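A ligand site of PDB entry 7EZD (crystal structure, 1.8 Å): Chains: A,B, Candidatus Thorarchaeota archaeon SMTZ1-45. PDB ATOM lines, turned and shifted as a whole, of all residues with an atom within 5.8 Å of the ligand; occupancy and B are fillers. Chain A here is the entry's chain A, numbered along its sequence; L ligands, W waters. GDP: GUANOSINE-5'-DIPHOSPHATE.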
ATOM      1  N   GLY A  13       0.727 -22.782  -0.386  1.00  0.00           N
ATOM      2  CA  GLY A  13       1.126 -22.543   0.986  1.00  0.00           C
ATOM      3  C   GLY A  13       2.308 -23.398   1.399  1.00  0.00           C
ATOM      4  O   GLY A  13       2.644 -24.399   0.756  1.00  0.00           O
ATOM      5  N   ASP A  14       2.936 -22.997   2.497  1.00  0.00           N
ATOM      6  CA  ASP A  14       4.139 -23.658   2.984  1.00  0.00           C
ATOM      7  C   ASP A  14       3.848 -25.104   3.366  1.00  0.00           C
ATOM      8  O   ASP A  14       2.701 -25.543   3.461  1.00  0.00           O
ATOM      9  CB  ASP A  14       4.702 -22.911   4.197  1.00  0.00           C
ATOM     10  CG  ASP A  14       5.442 -21.640   3.830  1.00  0.00           C
ATOM     11  OD1 ASP A  14       5.508 -21.315   2.625  1.00  0.00           O
ATOM     12  OD2 ASP A  14       5.964 -20.986   4.746  1.00  0.00           O
ATOM     13  N   GLY A  15       4.923 -25.854   3.587  1.00  0.00           N
ATOM     14  CA  GLY A  15       4.764 -27.229   4.031  1.00  0.00           C
ATOM     15  C   GLY A  15       4.036 -27.290   5.365  1.00  0.00           C
ATOM     16  O   GLY A  15       4.231 -26.448   6.238  1.00  0.00           O
ATOM     17  N   ALA A  16       3.158 -28.290   5.486  1.00  0.00           N
ATOM     18  CA  ALA A  16       2.432 -28.607   6.717  1.00  0.00           C
ATOM     19  C   ALA A  16       1.429 -27.534   7.139  1.00  0.00           C
ATOM     20  O   ALA A  16       1.025 -27.483   8.312  1.00  0.00           O
ATOM     21  CB  ALA A  16       3.402 -28.896   7.872  1.00  0.00           C
ATOM     22  N   VAL A  17       0.988 -26.668   6.208  1.00  0.00           N
ATOM     23  CA  VAL A  17      -0.086 -25.743   6.543  1.00  0.00           C
ATOM     24  C   VAL A  17      -1.450 -26.414   6.453  1.00  0.00           C
ATOM     25  O   VAL A  17      -2.434 -25.894   7.001  1.00  0.00           O
ATOM     26  CB  VAL A  17      -0.071 -24.481   5.664  1.00  0.00           C
ATOM     27  CG1 VAL A  17       1.269 -23.729   5.805  1.00  0.00           C
ATOM     28  CG2 VAL A  17      -0.371 -24.834   4.197  1.00  0.00           C
ATOM     29  N   GLY A  18      -1.539 -27.558   5.777  1.00  0.00           N
ATOM     30  CA  GLY A  18      -2.780 -28.307   5.722  1.00  0.00           C
ATOM     31  C   GLY A  18      -3.385 -28.437   4.342  1.00  0.00           C
ATOM     32  O   GLY A  18      -4.593 -28.685   4.216  1.00  0.00           O
ATOM     33  N   LYS A  19      -2.570 -28.266   3.292  1.00  0.00           N
ATOM     34  CA  LYS A  19      -3.082 -28.361   1.930  1.00  0.00           C
ATOM     35  C   LYS A  19      -3.700 -29.737   1.662  1.00  0.00           C
ATOM     36  O   LYS A  19      -4.823 -29.834   1.155  1.00  0.00           O
ATOM     37  CB  LYS A  19      -1.962 -28.070   0.930  1.00  0.00           C
ATOM     38  CG  LYS A  19      -1.400 -26.657   1.021  1.00  0.00           C
ATOM     39  CD  LYS A  19      -0.309 -26.442  -0.025  1.00  0.00           C
ATOM     40  CE  LYS A  19       0.837 -27.429   0.125  1.00  0.00           C
ATOM     41  NZ  LYS A  19       1.594 -27.256   1.403  1.00  0.00           N
ATOM     42  N   THR A  20      -2.980 -30.806   2.010  1.00  0.00           N
ATOM     43  CA  THR A  20      -3.520 -32.150   1.801  1.00  0.00           C
ATOM     44  C   THR A  20      -4.744 -32.393   2.669  1.00  0.00           C
ATOM     45  O   THR A  20      -5.780 -32.863   2.196  1.00  0.00           O
ATOM     46  CB  THR A  20      -2.440 -33.198   2.091  1.00  0.00           C
ATOM     47  OG1 THR A  20      -1.301 -32.951   1.264  1.00  0.00           O
ATOM     48  CG2 THR A  20      -2.960 -34.586   1.797  1.00  0.00           C
ATOM     49  N   ALA A  21      -4.647 -32.060   3.960  1.00  0.00           N
ATOM     50  CA  ALA A  21      -5.759 -32.286   4.883  1.00  0.00           C
ATOM     51  C   ALA A  21      -7.013 -31.533   4.437  1.00  0.00           C
ATOM     52  O   ALA A  21      -8.124 -32.049   4.555  1.00  0.00           O
ATOM     53  CB  ALA A  21      -5.354 -31.879   6.295  1.00  0.00           C
ATOM     54  N   MET A  22      -6.841 -30.304   3.943  1.00  0.00           N
ATOM     55  CA  MET A  22      -8.002 -29.563   3.462  1.00  0.00           C
ATOM     56  C   MET A  22      -8.607 -30.238   2.230  1.00  0.00           C
ATOM     57  O   MET A  22      -9.834 -30.347   2.113  1.00  0.00           O
ATOM     58  CB  MET A  22      -7.612 -28.124   3.155  1.00  0.00           C
ATOM     59  CG  MET A  22      -8.800 -27.243   2.832  1.00  0.00           C
ATOM     60  SD  MET A  22      -8.394 -25.486   2.849  1.00  0.00           S
ATOM     61  CE  MET A  22     -10.036 -24.781   2.780  1.00  0.00           C
ATOM     62  N   PHE A  31     -10.822 -36.690   8.275  1.00  0.00           N
ATOM     63  CA  PHE A  31      -9.522 -36.200   8.727  1.00  0.00           C
ATOM     64  C   PHE A  31      -8.794 -37.318   9.434  1.00  0.00           C
ATOM     65  O   PHE A  31      -9.406 -38.075  10.198  1.00  0.00           O
ATOM     66  CB  PHE A  31      -9.708 -34.998   9.659  1.00  0.00           C
ATOM     67  CG  PHE A  31      -8.420 -34.442  10.212  1.00  0.00           C
ATOM     68  CD1 PHE A  31      -7.954 -34.846  11.460  1.00  0.00           C
ATOM     69  CD2 PHE A  31      -7.710 -33.472   9.516  1.00  0.00           C
ATOM     70  CE1 PHE A  31      -6.790 -34.314  11.976  1.00  0.00           C
ATOM     71  CE2 PHE A  31      -6.541 -32.949  10.030  1.00  0.00           C
ATOM     72  CZ  PHE A  31      -6.082 -33.367  11.272  1.00  0.00           C
ATOM     73  N   ASP A  32      -7.494 -37.436   9.186  1.00  0.00           N
ATOM     74  CA  ASP A  32      -6.684 -38.503   9.793  1.00  0.00           C
ATOM     75  C   ASP A  32      -5.266 -37.993   9.914  1.00  0.00           C
ATOM     76  O   ASP A  32      -4.651 -37.638   8.904  1.00  0.00           O
ATOM     77  CB  ASP A  32      -6.738 -39.782   8.954  1.00  0.00           C
ATOM     78  CG  ASP A  32      -6.193 -41.016   9.695  1.00  0.00           C
ATOM     79  OD1 ASP A  32      -5.394 -40.852  10.638  1.00  0.00           O
ATOM     80  OD2 ASP A  32      -6.560 -42.145   9.314  1.00  0.00           O
ATOM     81  N   THR A  33      -4.735 -37.957  11.148  1.00  0.00           N
ATOM     82  CA  THR A  33      -3.344 -37.570  11.362  1.00  0.00           C
ATOM     83  C   THR A  33      -2.405 -38.459  10.564  1.00  0.00           C
ATOM     84  O   THR A  33      -1.308 -38.029  10.181  1.00  0.00           O
ATOM     85  CB  THR A  33      -3.011 -37.640  12.849  1.00  0.00           C
ATOM     86  OG1 THR A  33      -3.935 -36.833  13.579  1.00  0.00           O
ATOM     87  CG2 THR A  33      -1.595 -37.123  13.117  1.00  0.00           C
ATOM     88  N   ARG A  37      -0.476 -39.572   1.778  1.00  0.00           N
ATOM     89  CA  ARG A  37      -0.760 -39.023   0.460  1.00  0.00           C
ATOM     90  C   ARG A  37       0.049 -39.751  -0.600  1.00  0.00           C
ATOM     91  O   ARG A  37       0.943 -40.538  -0.273  1.00  0.00           O
ATOM     92  CB  ARG A  37      -0.448 -37.524   0.411  1.00  0.00           C
ATOM     93  CG  ARG A  37       1.037 -37.178   0.558  1.00  0.00           C
ATOM     94  CD  ARG A  37       1.409 -36.910   2.009  1.00  0.00           C
ATOM     95  NE  ARG A  37       0.884 -35.625   2.498  1.00  0.00           N
ATOM     96  CZ  ARG A  37       1.634 -34.626   2.945  1.00  0.00           C
ATOM     97  NH1 ARG A  37       1.064 -33.501   3.358  1.00  0.00           N
ATOM     98  NH2 ARG A  37       2.961 -34.750   2.999  1.00  0.00           N
ATOM     99  N   ASP A  63      -1.949 -30.100  -5.967  1.00  0.00           N
ATOM    100  CA  ASP A  63      -1.223 -29.926  -4.719  1.00  0.00           C
ATOM    101  C   ASP A  63       0.210 -30.408  -4.912  1.00  0.00           C
ATOM    102  O   ASP A  63       0.422 -31.539  -5.337  1.00  0.00           O
ATOM    103  CB  ASP A  63      -1.919 -30.713  -3.597  1.00  0.00           C
ATOM    104  CG  ASP A  63      -1.376 -30.364  -2.217  1.00  0.00           C
ATOM    105  OD1 ASP A  63      -0.387 -29.619  -2.125  1.00  0.00           O
ATOM    106  OD2 ASP A  63      -1.969 -30.853  -1.228  1.00  0.00           O
ATOM    107  N   ASN A 121      -5.793 -21.576   8.098  1.00  0.00           N
ATOM    108  CA  ASN A 121      -6.119 -22.949   8.480  1.00  0.00           C
ATOM    109  C   ASN A 121      -5.644 -23.263   9.895  1.00  0.00           C
ATOM    110  O   ASN A 121      -4.780 -22.577  10.447  1.00  0.00           O
ATOM    111  CB  ASN A 121      -5.517 -23.950   7.490  1.00  0.00           C
ATOM    112  CG  ASN A 121      -6.076 -25.351   7.655  1.00  0.00           C
ATOM    113  OD1 ASN A 121      -7.274 -25.528   7.865  1.00  0.00           O
ATOM    114  ND2 ASN A 121      -5.208 -26.355   7.587  1.00  0.00           N
ATOM    115  N   LYS A 122      -6.212 -24.340  10.462  1.00  0.00           N
ATOM    116  CA  LYS A 122      -5.895 -24.841  11.804  1.00  0.00           C
ATOM    117  C   LYS A 122      -6.438 -23.946  12.919  1.00  0.00           C
ATOM    118  O   LYS A 122      -5.871 -23.886  14.009  1.00  0.00           O
ATOM    119  CB  LYS A 122      -4.394 -25.047  12.002  1.00  0.00           C
ATOM    120  CG  LYS A 122      -3.742 -25.970  10.981  1.00  0.00           C
ATOM    121  CD  LYS A 122      -2.389 -26.465  11.502  1.00  0.00           C
ATOM    122  CE  LYS A 122      -1.563 -27.121  10.416  1.00  0.00           C
ATOM    123  NZ  LYS A 122      -0.226 -27.568  10.941  1.00  0.00           N
ATOM    124  N   VAL A 123      -7.552 -23.244  12.664  1.00  0.00           N
ATOM    125  CA  VAL A 123      -8.101 -22.345  13.680  1.00  0.00           C
ATOM    126  C   VAL A 123      -8.672 -23.101  14.872  1.00  0.00           C
ATOM    127  O   VAL A 123      -8.994 -22.485  15.900  1.00  0.00           O
ATOM    128  CB  VAL A 123      -9.166 -21.415  13.068  1.00  0.00           C
ATOM    129  CG1 VAL A 123      -8.561 -20.572  11.942  1.00  0.00           C
ATOM    130  CG2 VAL A 123     -10.359 -22.218  12.567  1.00  0.00           C
ATOM    131  N   ASP A 124      -8.794 -24.426  14.777  1.00  0.00           N
ATOM    132  CA  ASP A 124      -9.193 -25.211  15.941  1.00  0.00           C
ATOM    133  C   ASP A 124      -8.126 -25.203  17.022  1.00  0.00           C
ATOM    134  O   ASP A 124      -8.421 -25.527  18.172  1.00  0.00           O
ATOM    135  CB  ASP A 124      -9.505 -26.651  15.537  1.00  0.00           C
ATOM    136  CG  ASP A 124      -8.311 -27.342  14.909  1.00  0.00           C
ATOM    137  OD1 ASP A 124      -7.984 -27.021  13.742  1.00  0.00           O
ATOM    138  OD2 ASP A 124      -7.702 -28.207  15.576  1.00  0.00           O
ATOM    139  N   LEU A 125      -6.890 -24.854  16.676  1.00  0.00           N
ATOM    140  CA  LEU A 125      -5.773 -24.831  17.630  1.00  0.00           C
ATOM    141  C   LEU A 125      -5.703 -23.472  18.330  1.00  0.00           C
ATOM    142  O   LEU A 125      -4.766 -22.694  18.154  1.00  0.00           O
ATOM    143  CB  LEU A 125      -4.467 -25.159  16.915  1.00  0.00           C
ATOM    144  CG  LEU A 125      -4.324 -26.559  16.313  1.00  0.00           C
ATOM    145  CD1 LEU A 125      -3.028 -26.684  15.529  1.00  0.00           C
ATOM    146  CD2 LEU A 125      -4.386 -27.628  17.378  1.00  0.00           C
ATOM    147  N   SER A 150     -10.553 -21.634   8.499  1.00  0.00           N
ATOM    148  CA  SER A 150     -10.920 -23.016   8.251  1.00  0.00           C
ATOM    149  C   SER A 150     -10.194 -23.962   9.203  1.00  0.00           C
ATOM    150  O   SER A 150      -9.155 -23.625   9.787  1.00  0.00           O
ATOM    151  CB  SER A 150     -10.612 -23.437   6.810  1.00  0.00           C
ATOM    152  OG  SER A 150      -9.211 -23.594   6.628  1.00  0.00           O
ATOM    153  N   SER A 151     -10.753 -25.162   9.338  1.00  0.00           N
ATOM    154  CA  SER A 151     -10.084 -26.263  10.029  1.00  0.00           C
ATOM    155  C   SER A 151     -10.385 -27.539   9.268  1.00  0.00           C
ATOM    156  O   SER A 151     -11.545 -27.964   9.190  1.00  0.00           O
ATOM    157  CB  SER A 151     -10.540 -26.383  11.478  1.00  0.00           C
ATOM    158  OG  SER A 151     -10.078 -27.605  12.036  1.00  0.00           O
ATOM    159  N   ALA A 152      -9.346 -28.150   8.689  1.00  0.00           N
ATOM    160  CA  ALA A 152      -9.538 -29.465   8.079  1.00  0.00           C
ATOM    161  C   ALA A 152      -9.953 -30.499   9.115  1.00  0.00           C
ATOM    162  O   ALA A 152     -10.713 -31.425   8.801  1.00  0.00           O
ATOM    163  CB  ALA A 152      -8.243 -29.905   7.379  1.00  0.00           C
ATOM    164  N   LEU A 153      -9.504 -30.338  10.369  1.00  0.00           N
ATOM    165  CA  LEU A 153      -9.837 -31.307  11.414  1.00  0.00           C
ATOM    166  C   LEU A 153     -11.332 -31.301  11.702  1.00  0.00           C
ATOM    167  O   LEU A 153     -11.989 -32.350  11.671  1.00  0.00           O
ATOM    168  CB  LEU A 153      -9.030 -31.001  12.678  1.00  0.00           C
ATOM    169  CG  LEU A 153      -9.030 -32.048  13.810  1.00  0.00           C
ATOM    170  CD1 LEU A 153      -7.788 -31.893  14.667  1.00  0.00           C
ATOM    171  CD2 LEU A 153     -10.292 -31.943  14.679  1.00  0.00           C
ATOM    172  N   THR A 154     -11.889 -30.130  12.026  1.00  0.00           N
ATOM    173  CA  THR A 154     -13.312 -30.071  12.362  1.00  0.00           C
ATOM    174  C   THR A 154     -14.190 -29.950  11.132  1.00  0.00           C
ATOM    175  O   THR A 154     -15.406 -30.174  11.232  1.00  0.00           O
ATOM    176  CB  THR A 154     -13.590 -28.895  13.287  1.00  0.00           C
ATOM    177  OG1 THR A 154     -13.413 -27.667  12.566  1.00  0.00           O
ATOM    178  CG2 THR A 154     -12.655 -28.914  14.502  1.00  0.00           C
HETATM  179  PB  GDP L   1       0.442 -29.938   3.745  1.00  0.00           P
HETATM  180  O1B GDP L   1       0.267 -28.487   3.473  1.00  0.00           O
HETATM  181  O2B GDP L   1      -0.198 -30.786   2.725  1.00  0.00           O
HETATM  182  O3B GDP L   1       2.003 -30.258   3.923  1.00  0.00           O
HETATM  183  O3A GDP L   1      -0.172 -30.182   5.217  1.00  0.00           O
HETATM  184  PA  GDP L   1      -0.785 -31.545   5.775  1.00  0.00           P
HETATM  185  O1A GDP L   1      -2.106 -31.847   5.172  1.00  0.00           O
HETATM  186  O2A GDP L   1       0.209 -32.642   5.641  1.00  0.00           O
HETATM  187  O5' GDP L   1      -0.963 -31.154   7.322  1.00  0.00           O
HETATM  188  C5' GDP L   1       0.156 -30.996   8.173  1.00  0.00           C
HETATM  189  C4' GDP L   1      -0.153 -31.456   9.589  1.00  0.00           C
HETATM  190  O4' GDP L   1      -1.132 -30.616  10.164  1.00  0.00           O
HETATM  191  C3' GDP L   1      -0.740 -32.857   9.610  1.00  0.00           C
HETATM  192  O3' GDP L   1      -0.314 -33.468  10.806  1.00  0.00           O
HETATM  193  C2' GDP L   1      -2.233 -32.627   9.687  1.00  0.00           C
HETATM  194  O2' GDP L   1      -2.885 -33.703  10.318  1.00  0.00           O
HETATM  195  C1' GDP L   1      -2.304 -31.342  10.498  1.00  0.00           C
HETATM  196  N9  GDP L   1      -3.457 -30.496  10.150  1.00  0.00           N
HETATM  197  C8  GDP L   1      -3.853 -30.100   8.901  1.00  0.00           C
HETATM  198  N7  GDP L   1      -4.936 -29.302   9.027  1.00  0.00           N
HETATM  199  C5  GDP L   1      -5.232 -29.173  10.341  1.00  0.00           C
HETATM  200  C6  GDP L   1      -6.226 -28.500  11.027  1.00  0.00           C
HETATM  201  O6  GDP L   1      -7.067 -27.829  10.426  1.00  0.00           O
HETATM  202  N1  GDP L   1      -6.259 -28.563  12.406  1.00  0.00           N
HETATM  203  C2  GDP L   1      -5.322 -29.302  13.100  1.00  0.00           C
HETATM  204  N2  GDP L   1      -5.382 -29.361  14.436  1.00  0.00           N
HETATM  205  N3  GDP L   1      -4.348 -29.986  12.414  1.00  0.00           N
HETATM  206  C4  GDP L   1      -4.302 -29.921  11.062  1.00  0.00           C
HETATM  207  O   HOH W   1       0.245 -35.952  10.437  1.00  0.00           O
HETATM  208  O   HOH W   2      -2.881 -34.650   5.643  1.00  0.00           O
HETATM  209  O   HOH W   3       0.941 -30.829   0.029  1.00  0.00           O
HETATM  210  O   HOH W   4      -4.381 -31.279  16.107  1.00  0.00           O
HETATM  211  O   HOH W   5       0.284 -32.127  13.028  1.00  0.00           O
HETATM  212  O   HOH W   6      -3.917 -35.007   8.064  1.00  0.00           O
HETATM  213  O   HOH W   7       0.593 -35.120   7.041  1.00  0.00           O
HETATM  214  O   HOH W   8       3.460 -31.957   5.605  1.00  0.00           O
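Water W1 lies within hydrogen-bond range of an oxygen (O3') of the ligand (2.6 Å) and the backbone carbonyl oxygen (O) of Thr 33 (2.6 Å). Water W6 lies within hydrogen-bond range of O2' of the ligand (2.8 Å) and O of Asp 32 (2.9 Å). Water W3 lies within hydrogen-bond range of the side-chain carboxylate (OD1) of Asp 63 (2.8 Å), an oxygen (O2B) of the ligand (2.9 Å) and the side-chain hydroxyl (OG1) of Thr 20 (3.3 Å).
Residues that only touch the ligand: Phe 31, Leu 125, Asp 14 and Gly 15. The nearest printed residue that does not touch the ligand is Thr 33 (4.03 Å).
The guanidinium group (NH1) of Arg 37 sits at hydrogen-bond distance from the side-chain hydroxyl (OG1) of Thr 20 (3.2 Å). OD1 of Asp 124 sits at hydrogen-bond distance from OG of Ser 151, 2.8 Å away. The backbone carbonyl oxygen (O) of Ala 16 sits at hydrogen-bond distance from the side-chain amino group (NZ) of Lys 122, 2.9 Å away. The side-chain carboxylate of Asp 63 lies within hydrogen-bond range of the side-chain hydroxyl of Thr 20. N of Ala 152 lies within hydrogen-bond range of OD1 of Asn 121 (3.4 Å). N of Lys 122 sits at hydrogen-bond distance from O of Ser 150, at 3.1 Å. The backbone carbonyl oxygen (O) of Val 17 sits at hydrogen-bond distance from the side-chain amide nitrogen (ND2) of Asn 121. The side-chain amide oxygen (OD1) of Asn 121 lies within hydrogen-bond range of the side-chain hydroxyl (OG) of Ser 150 (3.0 Å).
The guanidinium group (NH1) of Arg 37 lies within salt-bridge range of an oxygen (O2A) of the ligand (2.6 Å). The side-chain carboxylate of Asp 124 sits at hydrogen-bond distance from a nitrogen (N1) of the ligand (2.7 Å). An oxygen (O1B) of the ligand lies within hydrogen-bond range of the backbone NH (N) of Lys 19. NZ of Lys 19 lies within salt-bridge range of O1B of the ligand (2.7 Å). The backbone NH (N) of Ala 16 lies within hydrogen-bond range of an oxygen (O3B) of the ligand, 2.8 Å away. O1A of the ligand lies within hydrogen-bond range of N of Ala 21, at 2.8 Å. N of Thr 20 sits at hydrogen-bond distance from O2B of the ligand. O2B of the ligand lies within hydrogen-bond range of OG1 of Thr 20 (2.8 Å). An oxygen (O6) of the ligand lies within hydrogen-bond range of the backbone NH (N) of Ala 152, 2.9 Å away. The backbone NH of Gly 18 is in hydrogen-bond range of an oxygen (O3A) of the ligand (3.0 Å). The side-chain amino group (NZ) of Lys 122 lies within hydrogen-bond range of an oxygen (O4') of the ligand, 3.3 Å away. The side-chain amide nitrogen (ND2) of Asn 121 sits at hydrogen-bond distance from a nitrogen (N7) of the ligand (3.3 Å). O1B of the ligand lies within hydrogen-bond range of N of Val 17, 3.4 Å away. The side-chain hydroxyl of Ser 151 sits at hydrogen-bond distance from an oxygen (O6) of the ligand. N of Leu 153 lies within hydrogen-bond range of O6 of the ligand (3.5 Å).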
